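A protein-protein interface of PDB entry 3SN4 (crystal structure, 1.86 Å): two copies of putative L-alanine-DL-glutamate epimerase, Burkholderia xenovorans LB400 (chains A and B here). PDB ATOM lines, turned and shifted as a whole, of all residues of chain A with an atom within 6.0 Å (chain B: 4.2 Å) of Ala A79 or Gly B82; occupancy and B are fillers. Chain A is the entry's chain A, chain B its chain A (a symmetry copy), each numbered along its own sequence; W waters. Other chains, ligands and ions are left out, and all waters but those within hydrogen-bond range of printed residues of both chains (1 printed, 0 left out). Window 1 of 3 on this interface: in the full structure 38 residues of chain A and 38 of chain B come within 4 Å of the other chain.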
ATOM      1  N   THR A  76      13.932  16.649  -1.356  1.00  0.00           N
ATOM      2  CA  THR A  76      14.504  16.767  -0.013  1.00  0.00           C
ATOM      3  C   THR A  76      13.487  17.214   1.051  1.00  0.00           C
ATOM      4  O   THR A  76      13.875  17.641   2.164  1.00  0.00           O
ATOM      5  CB  THR A  76      15.726  17.724   0.001  1.00  0.00           C
ATOM      6  OG1 THR A  76      15.317  19.036  -0.365  1.00  0.00           O
ATOM      7  CG2 THR A  76      16.816  17.252  -0.962  1.00  0.00           C
ATOM      8  N   ARG A  77      12.196  17.114   0.723  1.00  0.00           N
ATOM      9  CA  ARG A  77      11.109  17.646   1.573  1.00  0.00           C
ATOM     10  C   ARG A  77      11.215  17.211   3.059  1.00  0.00           C
ATOM     11  O   ARG A  77      11.077  18.043   3.923  1.00  0.00           O
ATOM     12  CB  ARG A  77       9.757  17.210   1.010  1.00  0.00           C
ATOM     13  CG  ARG A  77       8.647  18.251   1.062  1.00  0.00           C
ATOM     14  CD  ARG A  77       7.374  17.684   0.420  1.00  0.00           C
ATOM     15  NE  ARG A  77       6.458  18.770   0.113  1.00  0.00           N
ATOM     16  CZ  ARG A  77       6.165  19.241  -1.085  1.00  0.00           C
ATOM     17  NH1 ARG A  77       6.620  18.688  -2.189  1.00  0.00           N
ATOM     18  NH2 ARG A  77       5.345  20.275  -1.166  1.00  0.00           N
ATOM     19  N   PRO A  78      11.479  15.915   3.338  1.00  0.00           N
ATOM     20  CA  PRO A  78      11.558  15.479   4.729  1.00  0.00           C
ATOM     21  C   PRO A  78      12.614  16.150   5.585  1.00  0.00           C
ATOM     22  O   PRO A  78      12.404  16.302   6.816  1.00  0.00           O
ATOM     23  CB  PRO A  78      11.821  13.980   4.614  1.00  0.00           C
ATOM     24  CG  PRO A  78      11.279  13.627   3.326  1.00  0.00           C
ATOM     25  CD  PRO A  78      11.600  14.759   2.438  1.00  0.00           C
ATOM     26  N   ALA A  79      13.715  16.577   4.976  1.00  0.00           N
ATOM     27  CA  ALA A  79      14.814  17.177   5.734  1.00  0.00           C
ATOM     28  C   ALA A  79      15.080  18.623   5.295  1.00  0.00           C
ATOM     29  O   ALA A  79      16.202  19.115   5.371  1.00  0.00           O
ATOM     30  CB  ALA A  79      16.079  16.299   5.606  1.00  0.00           C
ATOM     31  N   THR A  80      14.028  19.305   4.855  1.00  0.00           N
ATOM     32  CA  THR A  80      14.152  20.682   4.399  1.00  0.00           C
ATOM     33  C   THR A  80      14.577  21.608   5.528  1.00  0.00           C
ATOM     34  O   THR A  80      14.438  21.299   6.734  1.00  0.00           O
ATOM     35  CB  THR A  80      12.854  21.215   3.725  1.00  0.00           C
ATOM     36  OG1 THR A  80      13.159  22.406   2.970  1.00  0.00           O
ATOM     37  CG2 THR A  80      11.768  21.514   4.769  1.00  0.00           C
ATOM     38  N   GLY A  81      15.082  22.758   5.117  1.00  0.00           N
ATOM     39  CA  GLY A  81      15.685  23.687   6.025  1.00  0.00           C
ATOM     40  C   GLY A  81      17.163  23.425   6.122  1.00  0.00           C
ATOM     41  O   GLY A  81      17.696  22.515   5.492  1.00  0.00           O
ATOM     42  N   GLY A  82      17.815  24.243   6.936  1.00  0.00           N
ATOM     43  CA  GLY A  82      19.204  24.024   7.327  1.00  0.00           C
ATOM     44  C   GLY A  82      20.137  23.802   6.155  1.00  0.00           C
ATOM     45  O   GLY A  82      20.068  24.504   5.143  1.00  0.00           O
ATOM     46  N   VAL A  84      20.370  21.428   3.982  1.00  0.00           N
ATOM     47  CA  VAL A  84      19.711  21.053   2.717  1.00  0.00           C
ATOM     48  C   VAL A  84      19.300  22.328   1.963  1.00  0.00           C
ATOM     49  O   VAL A  84      19.650  22.535   0.801  1.00  0.00           O
ATOM     50  CB  VAL A  84      18.477  20.106   2.949  1.00  0.00           C
ATOM     51  CG1 VAL A  84      17.521  20.126   1.742  1.00  0.00           C
ATOM     52  CG2 VAL A  84      18.937  18.673   3.240  1.00  0.00           C
ATOM     53  N   SER A  85      18.599  23.224   2.646  1.00  0.00           N
ATOM     54  CA  SER A  85      18.120  24.437   2.004  1.00  0.00           C
ATOM     55  C   SER A  85      19.261  25.357   1.602  1.00  0.00           C
ATOM     56  O   SER A  85      19.159  26.043   0.584  1.00  0.00           O
ATOM     57  CB  SER A  85      17.097  25.162   2.871  1.00  0.00           C
ATOM     58  OG  SER A  85      15.891  24.416   2.933  1.00  0.00           O
ATOM     59  N   GLY B  42      15.481  11.994   1.656  1.00  0.00           N
ATOM     60  CA  GLY B  42      15.643  13.429   1.477  1.00  0.00           C
ATOM     61  C   GLY B  42      16.852  14.050   2.146  1.00  0.00           C
ATOM     62  O   GLY B  42      16.886  15.265   2.302  1.00  0.00           O
ATOM     63  N   SER B  43      17.862  13.236   2.496  1.00  0.00           N
ATOM     64  CA  SER B  43      18.828  13.656   3.521  1.00  0.00           C
ATOM     65  C   SER B  43      20.328  13.494   3.123  1.00  0.00           C
ATOM     66  O   SER B  43      21.107  12.876   3.840  1.00  0.00           O
ATOM     67  CB  SER B  43      18.521  12.896   4.828  1.00  0.00           C
ATOM     68  OG  SER B  43      17.268  13.253   5.440  1.00  0.00           O
ATOM     69  N   GLY B  81      18.278  21.450  12.925  1.00  0.00           N
ATOM     70  CA  GLY B  81      17.237  20.751  12.235  1.00  0.00           C
ATOM     71  C   GLY B  81      17.820  19.935  11.114  1.00  0.00           C
ATOM     72  O   GLY B  81      19.026  19.937  10.879  1.00  0.00           O
ATOM     73  N   GLY B  82      16.931  19.240  10.417  1.00  0.00           N
ATOM     74  CA  GLY B  82      17.265  18.559   9.170  1.00  0.00           C
ATOM     75  C   GLY B  82      18.479  17.660   9.276  1.00  0.00           C
ATOM     76  O   GLY B  82      18.637  16.912  10.243  1.00  0.00           O
ATOM     77  N   VAL B  83      19.354  17.759   8.292  1.00  0.00           N
ATOM     78  CA  VAL B  83      20.451  16.794   8.201  1.00  0.00           C
ATOM     79  C   VAL B  83      21.464  17.042   9.296  1.00  0.00           C
ATOM     80  O   VAL B  83      22.096  16.108   9.734  1.00  0.00           O
ATOM     81  CB  VAL B  83      21.113  16.704   6.817  1.00  0.00           C
ATOM     82  CG1 VAL B  83      20.113  16.360   5.719  1.00  0.00           C
ATOM     83  CG2 VAL B  83      21.842  17.937   6.486  1.00  0.00           C
ATOM     84  N   VAL B  84      21.606  18.280   9.779  1.00  0.00           N
ATOM     85  CA  VAL B  84      22.482  18.541  10.936  1.00  0.00           C
ATOM     86  C   VAL B  84      21.969  17.749  12.150  1.00  0.00           C
ATOM     87  O   VAL B  84      22.697  16.979  12.775  1.00  0.00           O
ATOM     88  CB  VAL B  84      22.592  20.076  11.263  1.00  0.00           C
ATOM     89  CG1 VAL B  84      23.066  20.307  12.710  1.00  0.00           C
ATOM     90  CG2 VAL B  84      23.532  20.777  10.276  1.00  0.00           C
ATOM     91  N   SER B  85      20.685  17.890  12.452  1.00  0.00           N
ATOM     92  CA  SER B  85      20.120  17.223  13.614  1.00  0.00           C
ATOM     93  C   SER B  85      20.110  15.710  13.453  1.00  0.00           C
ATOM     94  O   SER B  85      20.273  14.994  14.441  1.00  0.00           O
ATOM     95  CB  SER B  85      18.731  17.757  13.944  1.00  0.00           C
ATOM     96  OG  SER B  85      18.822  19.086  14.437  1.00  0.00           O
ATOM     97  N   GLU B  86      19.971  15.236  12.218  1.00  0.00           N
ATOM     98  CA  GLU B  86      20.131  13.800  11.925  1.00  0.00           C
ATOM     99  C   GLU B  86      21.510  13.248  12.274  1.00  0.00           C
ATOM    100  O   GLU B  86      21.606  12.118  12.770  1.00  0.00           O
ATOM    101  CB  GLU B  86      19.855  13.484  10.462  1.00  0.00           C
ATOM    102  CG  GLU B  86      18.392  13.467  10.084  1.00  0.00           C
ATOM    103  CD  GLU B  86      18.180  13.135   8.626  1.00  0.00           C
ATOM    104  OE1 GLU B  86      18.601  12.036   8.181  1.00  0.00           O
ATOM    105  OE2 GLU B  86      17.616  13.987   7.891  1.00  0.00           O
ATOM    106  N   PHE B 272      11.768  17.661  14.345  1.00  0.00           N
ATOM    107  CA  PHE B 272      12.874  17.602  15.324  1.00  0.00           C
ATOM    108  C   PHE B 272      12.638  18.411  16.597  1.00  0.00           C
ATOM    109  O   PHE B 272      12.489  19.633  16.548  1.00  0.00           O
ATOM    110  CB  PHE B 272      14.167  18.140  14.698  1.00  0.00           C
ATOM    111  CG  PHE B 272      14.678  17.333  13.526  1.00  0.00           C
ATOM    112  CD1 PHE B 272      15.649  16.366  13.707  1.00  0.00           C
ATOM    113  CD2 PHE B 272      14.204  17.573  12.236  1.00  0.00           C
ATOM    114  CE1 PHE B 272      16.114  15.653  12.626  1.00  0.00           C
ATOM    115  CE2 PHE B 272      14.664  16.843  11.168  1.00  0.00           C
ATOM    116  CZ  PHE B 272      15.622  15.894  11.370  1.00  0.00           C
HETATM  117  O   HOH W   1      18.674  19.941   6.306  1.00  0.00           O
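The side-chain hydroxyl (OG) of Ser B43 is in hydrogen-bond range of the side-chain carboxylate (OE2) of Glu B86 (2.6 Å).
Thr A76 touches Gly B42.
Gly B42 touches Ala A79.
Ala A79 touches Ser B43.
Gly B82 touches Ala A79.
CB of Ala A79 touches OE2 of Glu B86, at 3.6 Å.
CG2 of Val A84 touches CG1 of Val B83 (3.6 Å).
Printed residues of chain B within 4 Å of Ala A79: Gly B42, Ser B43, Gly B82 and Glu B86.
Thr A80 touches none of the printed residues of chain B.
Printed residues of chain B within 4 Å of Val A84: Val B83.
Of the printed residues of chain A, Gly B42 touches Thr A76 (3.6 Å) and Ala A79 (3.6 Å).
Printed residues of chain A within 4 Å of Ser B43: Ala A79.
Printed residues of chain A within 4 Å of Gly B82: Ala A79 (3.98 Å).
Ser B85 touches none of the printed residues of chain A.
Printed residues of chain A within 4 Å of Glu B86: Ala A79.
The nearest printed residue of chain B that does not touch Ala A79 is Val B83 (4.04 Å).
The nearest printed residue of chain B that does not touch Val A84 is Gly B42 (4.1 Å).
Hydrophobic or aromatic side chains of chain B that line the printed part of chain A: Val B83.
Along chain B the printed residues that touch a printed residue of chain A span positions 42 to 86.
Of the 9 printed residues of chain A, 3 touch a printed residue of chain B.
Hydrophobic or aromatic side chains of chain A within 4 Å of the printed part of chain B: Ala A79 and Val A84.
Among the printed residues, no Asp or Glu carboxylate lies within 4 Å of a Lys or Arg side-chain nitrogen of the other chain.
Positions printed for both chains: 81, 82, 84 and 85.
Of the 6 pairs that touch across the chains among the printed residues, none has its exchanged pair printed and touching as well.
Water W1 lies within hydrogen-bond range of O of Ala A79 (2.8 Å), O of Gly A81 (2.9 Å), N of Val B83 (3.0 Å) and N of Val A84 (3.2 Å).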
